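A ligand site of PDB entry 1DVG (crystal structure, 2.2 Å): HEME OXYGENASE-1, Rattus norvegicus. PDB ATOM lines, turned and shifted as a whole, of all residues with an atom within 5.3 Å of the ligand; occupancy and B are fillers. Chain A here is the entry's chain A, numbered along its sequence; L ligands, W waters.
Lys 18 touches the ligand. Glu 29 touches the ligand. Met 34 touches the ligand. Gln 38 touches the ligand. Thr 135 touches the ligand (O to C25, 3.6 Å). Gly 139 touches the ligand (CA to C4, 3.6 Å). CB of Ser 142 touches O1 of the ligand, 3.5 Å away. Gly 143 touches the ligand (CA to C13, 3.7 Å). Leu 147 touches the ligand. Phe 207 touches the ligand (CZ to C4, 3.5 Å). Asn 210 touches the ligand. Phe 214 touches the ligand. Hydrophobic or aromatic side chains within 4 Å of the ligand: His 25, Met 34, Tyr 134, Leu 147, Phe 207 and Phe 214. Within 4 Å of the ligand: Lys 18, His 25, Glu 29, Met 34, Gln 38, Tyr 134, Thr 135, Gly 139, Ser 142, Gly 143, Leu 147, Lys 179, Arg 183, Phe 207, Asn 210 and Phe 214. The nearest printed residue that does not touch the ligand is Leu 138 (4.02 Å).
Water W2 lies within hydrogen-bond range of an oxygen (O3) of the ligand, the backbone carbonyl oxygen of Ser 14 and the guanidinium group of Arg 183. Water W4 lies within hydrogen-bond range of an oxygen (O4) of the ligand (2.7 Å) and the side-chain amino group (NZ) of Lys 18 (3.4 Å). Water W1 lies within hydrogen-bond range of the side-chain amino group of Lys 179 and an oxygen (O1) of the ligand. Water W3 lies within hydrogen-bond range of NZ of Lys 179 and NH2 of Arg 183. Water W6 lies within hydrogen-bond range of the backbone carbonyl oxygen (O) of Ser 142 (2.9 Å) and an oxygen (O1) of the ligand (3.3 Å).
The side-chain carboxylate of Glu 29 sits at hydrogen-bond distance from a ring nitrogen (ND1) of His 25 (2.9 Å). The side-chain amide nitrogen of Gln 38 is in hydrogen-bond range of the backbone carbonyl oxygen of Glu 29 (3.4 Å). The side-chain amide oxygen (OD1) of Asn 210 sits at hydrogen-bond distance from the guanidinium group (NH1) of Arg 136, at 2.8 Å. The side-chain hydroxyl (OG) of Ser 142 is in hydrogen-bond range of the side-chain amino group (NZ) of Lys 179. The backbone carbonyl oxygen of Leu 138 sits at hydrogen-bond distance from the side-chain hydroxyl of Ser 142 (2.4 Å).
A ring nitrogen (NE2) of His 25 binds an iron atom (FE1) of the ligand. The side-chain hydroxyl of Tyr 134 lies within hydrogen-bond range of an oxygen (O3) of the ligand, at 2.6 Å. NH2 of Arg 183 lies within salt-bridge range of O4 of the ligand, at 3.0 Å. An oxygen (O1) of the ligand is in salt-bridge range of the side-chain amino group (NZ) of Lys 179 (3.5 Å).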
ATOM      1  N   SER A  14      34.187 -14.252 -21.009  1.00  0.00           N
ATOM      2  CA  SER A  14      33.886 -14.927 -19.751  1.00  0.00           C
ATOM      3  C   SER A  14      35.029 -14.842 -18.755  1.00  0.00           C
ATOM      4  O   SER A  14      34.806 -14.704 -17.552  1.00  0.00           O
ATOM      5  CB  SER A  14      33.510 -16.387 -20.012  1.00  0.00           C
ATOM      6  OG  SER A  14      34.600 -17.118 -20.511  1.00  0.00           O
ATOM      7  N   LEU A  17      35.368 -11.152 -17.475  1.00  0.00           N
ATOM      8  CA  LEU A  17      34.338 -10.827 -16.484  1.00  0.00           C
ATOM      9  C   LEU A  17      34.713 -11.346 -15.112  1.00  0.00           C
ATOM     10  O   LEU A  17      34.573 -10.646 -14.105  1.00  0.00           O
ATOM     11  CB  LEU A  17      32.993 -11.425 -16.887  1.00  0.00           C
ATOM     12  CG  LEU A  17      32.213 -10.684 -17.970  1.00  0.00           C
ATOM     13  CD1 LEU A  17      31.083 -11.578 -18.468  1.00  0.00           C
ATOM     14  CD2 LEU A  17      31.685  -9.374 -17.410  1.00  0.00           C
ATOM     15  N   LYS A  18      35.193 -12.592 -15.057  1.00  0.00           N
ATOM     16  CA  LYS A  18      35.572 -13.190 -13.791  1.00  0.00           C
ATOM     17  C   LYS A  18      36.698 -12.419 -13.141  1.00  0.00           C
ATOM     18  O   LYS A  18      36.742 -12.248 -11.918  1.00  0.00           O
ATOM     19  CB  LYS A  18      36.016 -14.640 -14.008  1.00  0.00           C
ATOM     20  CG  LYS A  18      36.540 -15.301 -12.750  1.00  0.00           C
ATOM     21  CD  LYS A  18      36.578 -16.811 -12.886  1.00  0.00           C
ATOM     22  CE  LYS A  18      37.019 -17.468 -11.578  1.00  0.00           C
ATOM     23  NZ  LYS A  18      36.228 -17.000 -10.402  1.00  0.00           N
ATOM     24  N   THR A  21      35.417  -8.732 -11.915  1.00  0.00           N
ATOM     25  CA  THR A  21      34.512  -8.680 -10.765  1.00  0.00           C
ATOM     26  C   THR A  21      34.966  -9.416  -9.523  1.00  0.00           C
ATOM     27  O   THR A  21      34.215  -9.534  -8.558  1.00  0.00           O
ATOM     28  CB  THR A  21      33.127  -9.262 -11.122  1.00  0.00           C
ATOM     29  OG1 THR A  21      33.293 -10.640 -11.493  1.00  0.00           O
ATOM     30  CG2 THR A  21      32.494  -8.487 -12.247  1.00  0.00           C
ATOM     31  N   HIS A  25      33.209  -9.064  -5.936  1.00  0.00           N
ATOM     32  CA  HIS A  25      32.547 -10.303  -5.494  1.00  0.00           C
ATOM     33  C   HIS A  25      32.900 -10.519  -4.026  1.00  0.00           C
ATOM     34  O   HIS A  25      32.034 -10.836  -3.215  1.00  0.00           O
ATOM     35  CB  HIS A  25      33.003 -11.523  -6.314  1.00  0.00           C
ATOM     36  CG  HIS A  25      32.240 -12.773  -5.980  1.00  0.00           C
ATOM     37  ND1 HIS A  25      32.515 -13.552  -4.873  1.00  0.00           N
ATOM     38  CD2 HIS A  25      31.158 -13.335  -6.569  1.00  0.00           C
ATOM     39  CE1 HIS A  25      31.622 -14.527  -4.795  1.00  0.00           C
ATOM     40  NE2 HIS A  25      30.786 -14.413  -5.804  1.00  0.00           N
ATOM     41  N   ALA A  28      30.941  -8.383  -1.949  1.00  0.00           N
ATOM     42  CA  ALA A  28      29.559  -8.806  -1.813  1.00  0.00           C
ATOM     43  C   ALA A  28      29.447  -9.873  -0.734  1.00  0.00           C
ATOM     44  O   ALA A  28      28.477  -9.905   0.027  1.00  0.00           O
ATOM     45  CB  ALA A  28      29.043  -9.336  -3.135  1.00  0.00           C
ATOM     46  N   GLU A  29      30.445 -10.760  -0.655  1.00  0.00           N
ATOM     47  CA  GLU A  29      30.444 -11.813   0.351  1.00  0.00           C
ATOM     48  C   GLU A  29      30.685 -11.208   1.748  1.00  0.00           C
ATOM     49  O   GLU A  29      30.197 -11.744   2.748  1.00  0.00           O
ATOM     50  CB  GLU A  29      31.548 -12.832   0.083  1.00  0.00           C
ATOM     51  CG  GLU A  29      31.560 -13.443  -1.309  1.00  0.00           C
ATOM     52  CD  GLU A  29      32.782 -14.335  -1.520  1.00  0.00           C
ATOM     53  OE1 GLU A  29      32.842 -15.408  -0.900  1.00  0.00           O
ATOM     54  OE2 GLU A  29      33.685 -13.952  -2.302  1.00  0.00           O
ATOM     55  N   MET A  34      25.044 -10.699   3.748  1.00  0.00           N
ATOM     56  CA  MET A  34      25.510 -11.974   3.220  1.00  0.00           C
ATOM     57  C   MET A  34      26.356 -12.741   4.234  1.00  0.00           C
ATOM     58  O   MET A  34      26.190 -13.945   4.372  1.00  0.00           O
ATOM     59  CB  MET A  34      26.288 -11.776   1.920  1.00  0.00           C
ATOM     60  CG  MET A  34      25.426 -11.372   0.720  1.00  0.00           C
ATOM     61  SD  MET A  34      24.091 -12.697   0.157  1.00  0.00           S
ATOM     62  CE  MET A  34      22.526 -11.594   0.167  1.00  0.00           C
ATOM     63  N   GLN A  38      25.476 -16.605   5.171  1.00  0.00           N
ATOM     64  CA  GLN A  38      26.381 -17.753   5.067  1.00  0.00           C
ATOM     65  C   GLN A  38      26.576 -18.526   6.372  1.00  0.00           C
ATOM     66  O   GLN A  38      26.758 -19.737   6.349  1.00  0.00           O
ATOM     67  CB  GLN A  38      27.765 -17.326   4.586  1.00  0.00           C
ATOM     68  CG  GLN A  38      27.817 -16.687   3.239  1.00  0.00           C
ATOM     69  CD  GLN A  38      29.238 -16.371   2.825  1.00  0.00           C
ATOM     70  OE1 GLN A  38      30.052 -17.284   2.619  1.00  0.00           O
ATOM     71  NE2 GLN A  38      29.549 -15.075   2.716  1.00  0.00           N
ATOM     72  N   TYR A 134      24.618 -12.017 -16.533  1.00  0.00           N
ATOM     73  CA  TYR A 134      25.752 -12.757 -15.998  1.00  0.00           C
ATOM     74  C   TYR A 134      25.795 -12.667 -14.485  1.00  0.00           C
ATOM     75  O   TYR A 134      25.827 -13.671 -13.772  1.00  0.00           O
ATOM     76  CB  TYR A 134      27.040 -12.194 -16.586  1.00  0.00           C
ATOM     77  CG  TYR A 134      28.302 -12.467 -15.789  1.00  0.00           C
ATOM     78  CD1 TYR A 134      28.923 -13.712 -15.812  1.00  0.00           C
ATOM     79  CD2 TYR A 134      28.883 -11.454 -15.008  1.00  0.00           C
ATOM     80  CE1 TYR A 134      30.092 -13.941 -15.094  1.00  0.00           C
ATOM     81  CE2 TYR A 134      30.044 -11.678 -14.292  1.00  0.00           C
ATOM     82  CZ  TYR A 134      30.651 -12.915 -14.335  1.00  0.00           C
ATOM     83  OH  TYR A 134      31.843 -13.087 -13.672  1.00  0.00           O
ATOM     84  N   THR A 135      25.774 -11.427 -13.985  1.00  0.00           N
ATOM     85  CA  THR A 135      25.846 -11.153 -12.561  1.00  0.00           C
ATOM     86  C   THR A 135      24.766 -11.852 -11.776  1.00  0.00           C
ATOM     87  O   THR A 135      25.050 -12.462 -10.756  1.00  0.00           O
ATOM     88  CB  THR A 135      25.771  -9.640 -12.259  1.00  0.00           C
ATOM     89  OG1 THR A 135      26.850  -8.959 -12.918  1.00  0.00           O
ATOM     90  CG2 THR A 135      25.867  -9.385 -10.753  1.00  0.00           C
ATOM     91  N   ARG A 136      23.520 -11.762 -12.207  1.00  0.00           N
ATOM     92  CA  ARG A 136      22.473 -12.412 -11.446  1.00  0.00           C
ATOM     93  C   ARG A 136      22.411 -13.936 -11.660  1.00  0.00           C
ATOM     94  O   ARG A 136      22.505 -14.699 -10.700  1.00  0.00           O
ATOM     95  CB  ARG A 136      21.096 -11.794 -11.734  1.00  0.00           C
ATOM     96  CG  ARG A 136      20.741 -10.445 -11.061  1.00  0.00           C
ATOM     97  CD  ARG A 136      20.939 -10.418  -9.515  1.00  0.00           C
ATOM     98  NE  ARG A 136      20.475 -11.616  -8.844  1.00  0.00           N
ATOM     99  CZ  ARG A 136      20.608 -11.859  -7.546  1.00  0.00           C
ATOM    100  NH1 ARG A 136      21.184 -10.963  -6.754  1.00  0.00           N
ATOM    101  NH2 ARG A 136      20.169 -13.009  -7.031  1.00  0.00           N
ATOM    102  N   LEU A 138      24.555 -16.377 -13.097  1.00  0.00           N
ATOM    103  CA  LEU A 138      25.636 -17.263 -12.680  1.00  0.00           C
ATOM    104  C   LEU A 138      25.780 -17.270 -11.163  1.00  0.00           C
ATOM    105  O   LEU A 138      26.256 -18.253 -10.571  1.00  0.00           O
ATOM    106  CB  LEU A 138      26.958 -16.860 -13.346  1.00  0.00           C
ATOM    107  CG  LEU A 138      27.018 -16.920 -14.877  1.00  0.00           C
ATOM    108  CD1 LEU A 138      28.465 -17.203 -15.284  1.00  0.00           C
ATOM    109  CD2 LEU A 138      26.109 -17.998 -15.422  1.00  0.00           C
ATOM    110  N   GLY A 139      25.376 -16.170 -10.528  1.00  0.00           N
ATOM    111  CA  GLY A 139      25.433 -16.088  -9.076  1.00  0.00           C
ATOM    112  C   GLY A 139      24.386 -17.016  -8.484  1.00  0.00           C
ATOM    113  O   GLY A 139      24.637 -17.672  -7.471  1.00  0.00           O
ATOM    114  N   LEU A 141      23.329 -19.731  -9.725  1.00  0.00           N
ATOM    115  CA  LEU A 141      23.812 -21.098  -9.928  1.00  0.00           C
ATOM    116  C   LEU A 141      25.093 -21.408  -9.182  1.00  0.00           C
ATOM    117  O   LEU A 141      25.648 -22.501  -9.305  1.00  0.00           O
ATOM    118  CB  LEU A 141      24.051 -21.353 -11.421  1.00  0.00           C
ATOM    119  CG  LEU A 141      22.820 -21.284 -12.325  1.00  0.00           C
ATOM    120  CD1 LEU A 141      23.277 -21.342 -13.775  1.00  0.00           C
ATOM    121  CD2 LEU A 141      21.849 -22.420 -12.032  1.00  0.00           C
ATOM    122  N   SER A 142      25.582 -20.444  -8.410  1.00  0.00           N
ATOM    123  CA  SER A 142      26.816 -20.636  -7.653  1.00  0.00           C
ATOM    124  C   SER A 142      26.506 -20.439  -6.177  1.00  0.00           C
ATOM    125  O   SER A 142      25.979 -21.344  -5.529  1.00  0.00           O
ATOM    126  CB  SER A 142      27.861 -19.639  -8.117  1.00  0.00           C
ATOM    127  OG  SER A 142      27.968 -19.654  -9.534  1.00  0.00           O
ATOM    128  N   GLY A 143      26.805 -19.248  -5.660  1.00  0.00           N
ATOM    129  CA  GLY A 143      26.540 -18.947  -4.271  1.00  0.00           C
ATOM    130  C   GLY A 143      25.094 -19.254  -3.916  1.00  0.00           C
ATOM    131  O   GLY A 143      24.802 -19.737  -2.820  1.00  0.00           O
ATOM    132  N   LEU A 147      23.626 -21.007  -0.579  1.00  0.00           N
ATOM    133  CA  LEU A 147      22.638 -20.332   0.252  1.00  0.00           C
ATOM    134  C   LEU A 147      21.294 -21.046   0.347  1.00  0.00           C
ATOM    135  O   LEU A 147      20.652 -21.043   1.388  1.00  0.00           O
ATOM    136  CB  LEU A 147      22.429 -18.896  -0.251  1.00  0.00           C
ATOM    137  CG  LEU A 147      23.658 -17.979  -0.116  1.00  0.00           C
ATOM    138  CD1 LEU A 147      23.373 -16.628  -0.747  1.00  0.00           C
ATOM    139  CD2 LEU A 147      24.022 -17.797   1.343  1.00  0.00           C
ATOM    140  N   LYS A 179      26.864 -23.554 -16.461  1.00  0.00           N
ATOM    141  CA  LYS A 179      27.630 -22.305 -16.426  1.00  0.00           C
ATOM    142  C   LYS A 179      28.732 -22.345 -17.470  1.00  0.00           C
ATOM    143  O   LYS A 179      29.040 -21.328 -18.088  1.00  0.00           O
ATOM    144  CB  LYS A 179      28.232 -22.084 -15.028  1.00  0.00           C
ATOM    145  CG  LYS A 179      27.249 -21.466 -14.039  1.00  0.00           C
ATOM    146  CD  LYS A 179      27.372 -22.090 -12.666  1.00  0.00           C
ATOM    147  CE  LYS A 179      28.659 -21.716 -11.996  1.00  0.00           C
ATOM    148  NZ  LYS A 179      28.850 -22.549 -10.785  1.00  0.00           N
ATOM    149  N   ARG A 183      29.154 -19.694 -20.400  1.00  0.00           N
ATOM    150  CA  ARG A 183      30.396 -18.976 -20.685  1.00  0.00           C
ATOM    151  C   ARG A 183      30.739 -19.134 -22.161  1.00  0.00           C
ATOM    152  O   ARG A 183      31.169 -18.173 -22.816  1.00  0.00           O
ATOM    153  CB  ARG A 183      31.536 -19.511 -19.820  1.00  0.00           C
ATOM    154  CG  ARG A 183      31.367 -19.202 -18.347  1.00  0.00           C
ATOM    155  CD  ARG A 183      32.598 -19.582 -17.516  1.00  0.00           C
ATOM    156  NE  ARG A 183      32.335 -19.348 -16.094  1.00  0.00           N
ATOM    157  CZ  ARG A 183      31.940 -20.287 -15.247  1.00  0.00           C
ATOM    158  NH1 ARG A 183      31.783 -21.533 -15.670  1.00  0.00           N
ATOM    159  NH2 ARG A 183      31.687 -19.989 -13.980  1.00  0.00           N
ATOM    160  N   PHE A 207      27.294  -5.641  -9.622  1.00  0.00           N
ATOM    161  CA  PHE A 207      27.606  -6.119  -8.277  1.00  0.00           C
ATOM    162  C   PHE A 207      27.388  -4.985  -7.269  1.00  0.00           C
ATOM    163  O   PHE A 207      26.869  -5.206  -6.168  1.00  0.00           O
ATOM    164  CB  PHE A 207      29.066  -6.585  -8.194  1.00  0.00           C
ATOM    165  CG  PHE A 207      29.293  -8.025  -8.560  1.00  0.00           C
ATOM    166  CD1 PHE A 207      29.473  -8.408  -9.887  1.00  0.00           C
ATOM    167  CD2 PHE A 207      29.323  -9.005  -7.570  1.00  0.00           C
ATOM    168  CE1 PHE A 207      29.688  -9.742 -10.225  1.00  0.00           C
ATOM    169  CE2 PHE A 207      29.542 -10.349  -7.899  1.00  0.00           C
ATOM    170  CZ  PHE A 207      29.720 -10.715  -9.228  1.00  0.00           C
ATOM    171  N   ASN A 210      23.879  -4.623  -6.278  1.00  0.00           N
ATOM    172  CA  ASN A 210      23.475  -5.692  -5.354  1.00  0.00           C
ATOM    173  C   ASN A 210      24.031  -5.401  -3.957  1.00  0.00           C
ATOM    174  O   ASN A 210      23.355  -5.582  -2.961  1.00  0.00           O
ATOM    175  CB  ASN A 210      23.996  -7.034  -5.871  1.00  0.00           C
ATOM    176  CG  ASN A 210      23.115  -7.611  -6.954  1.00  0.00           C
ATOM    177  OD1 ASN A 210      22.147  -8.315  -6.660  1.00  0.00           O
ATOM    178  ND2 ASN A 210      23.426  -7.298  -8.213  1.00  0.00           N
ATOM    179  N   PHE A 214      21.965  -4.845  -0.503  1.00  0.00           N
ATOM    180  CA  PHE A 214      22.111  -5.618   0.729  1.00  0.00           C
ATOM    181  C   PHE A 214      22.356  -4.704   1.913  1.00  0.00           C
ATOM    182  O   PHE A 214      21.932  -4.998   3.037  1.00  0.00           O
ATOM    183  CB  PHE A 214      23.283  -6.610   0.670  1.00  0.00           C
ATOM    184  CG  PHE A 214      23.157  -7.622  -0.418  1.00  0.00           C
ATOM    185  CD1 PHE A 214      21.913  -8.176  -0.729  1.00  0.00           C
ATOM    186  CD2 PHE A 214      24.271  -8.020  -1.154  1.00  0.00           C
ATOM    187  CE1 PHE A 214      21.778  -9.102  -1.757  1.00  0.00           C
ATOM    188  CE2 PHE A 214      24.155  -8.939  -2.192  1.00  0.00           C
ATOM    189  CZ  PHE A 214      22.904  -9.481  -2.498  1.00  0.00           C
HETATM  190  C1  LIG L   1      30.703 -17.383  -8.429  1.00  0.00           C
HETATM  191  C2  LIG L   1      30.262 -18.019  -3.679  1.00  0.00           C
HETATM  192  C3  LIG L   1      27.446 -14.060  -3.502  1.00  0.00           C
HETATM  193  C4  LIG L   1      27.843 -13.543  -8.274  1.00  0.00           C
HETATM  194  C5  LIG L   1      30.839 -17.910  -7.161  1.00  0.00           C
HETATM  195  C6  LIG L   1      31.623 -19.101  -6.826  1.00  0.00           C
HETATM  196  C7  LIG L   1      31.476 -19.267  -5.470  1.00  0.00           C
HETATM  197  C8  LIG L   1      30.644 -18.210  -4.996  1.00  0.00           C
HETATM  198  C9  LIG L   1      32.090 -20.365  -4.606  1.00  0.00           C
HETATM  199  C10 LIG L   1      32.412 -19.926  -7.800  1.00  0.00           C
HETATM  200  C11 LIG L   1      31.555 -20.967  -8.605  1.00  0.00           C
HETATM  201  C12 LIG L   1      31.159 -22.152  -7.753  1.00  0.00           C
HETATM  202  O1  LIG L   1      29.974 -22.346  -7.448  1.00  0.00           O
HETATM  203  O2  LIG L   1      32.098 -22.949  -7.365  1.00  0.00           O
HETATM  204  C13 LIG L   1      29.455 -16.983  -3.205  1.00  0.00           C
HETATM  205  C14 LIG L   1      29.081 -16.765  -1.791  1.00  0.00           C
HETATM  206  C15 LIG L   1      28.311 -15.661  -1.750  1.00  0.00           C
HETATM  207  C16 LIG L   1      28.200 -15.193  -3.120  1.00  0.00           C
HETATM  208  C17 LIG L   1      29.530 -17.670  -0.667  1.00  0.00           C
HETATM  209  C18 LIG L   1      27.654 -14.985  -0.541  1.00  0.00           C
HETATM  210  C19 LIG L   1      26.696 -15.526   0.189  1.00  0.00           C
HETATM  211  C20 LIG L   1      27.277 -13.540  -4.787  1.00  0.00           C
HETATM  212  C21 LIG L   1      26.469 -12.383  -5.142  1.00  0.00           C
HETATM  213  C22 LIG L   1      26.584 -12.257  -6.497  1.00  0.00           C
HETATM  214  C23 LIG L   1      27.461 -13.322  -6.943  1.00  0.00           C
HETATM  215  C24 LIG L   1      25.678 -11.550  -4.146  1.00  0.00           C
HETATM  216  C25 LIG L   1      26.006 -11.292  -7.477  1.00  0.00           C
HETATM  217  C26 LIG L   1      25.191 -10.285  -7.260  1.00  0.00           C
HETATM  218  C27 LIG L   1      28.661 -14.528  -8.770  1.00  0.00           C
HETATM  219  C28 LIG L   1      29.031 -14.684 -10.143  1.00  0.00           C
HETATM  220  C29 LIG L   1      29.855 -15.791 -10.176  1.00  0.00           C
HETATM  221  C30 LIG L   1      29.973 -16.277  -8.819  1.00  0.00           C
HETATM  222  C31 LIG L   1      28.586 -13.810 -11.294  1.00  0.00           C
HETATM  223  C32 LIG L   1      30.499 -16.355 -11.417  1.00  0.00           C
HETATM  224  C33 LIG L   1      31.882 -15.693 -11.689  1.00  0.00           C
HETATM  225  C34 LIG L   1      32.536 -16.224 -12.907  1.00  0.00           C
HETATM  226  O3  LIG L   1      32.693 -15.524 -13.919  1.00  0.00           O
HETATM  227  O4  LIG L   1      32.919 -17.434 -12.895  1.00  0.00           O
HETATM  228  N1  LIG L   1      30.248 -17.378  -6.036  1.00  0.00           N
HETATM  229  N2  LIG L   1      28.886 -15.977  -3.993  1.00  0.00           N
HETATM  230  N3  LIG L   1      27.866 -14.078  -5.919  1.00  0.00           N
HETATM  231  N4  LIG L   1      29.232 -15.480  -7.976  1.00  0.00           N
HETATM  232 FE1  LIG L   1      29.103 -15.651  -6.035  1.00  0.00          FE
HETATM  233  O   HOH W   1      29.170 -24.798  -9.308  1.00  0.00           O
HETATM  234  O   HOH W   2      33.258 -16.603 -16.244  1.00  0.00           O
HETATM  235  O   HOH W   3      31.513 -21.830 -11.675  1.00  0.00           O
HETATM  236  O   HOH W   4      33.636 -19.157 -10.900  1.00  0.00           O
HETATM  237  O   HOH W   5      27.561 -16.640  -6.107  1.00  0.00           O
HETATM  238  O   HOH W   6      27.503 -23.771  -5.707  1.00  0.00           O
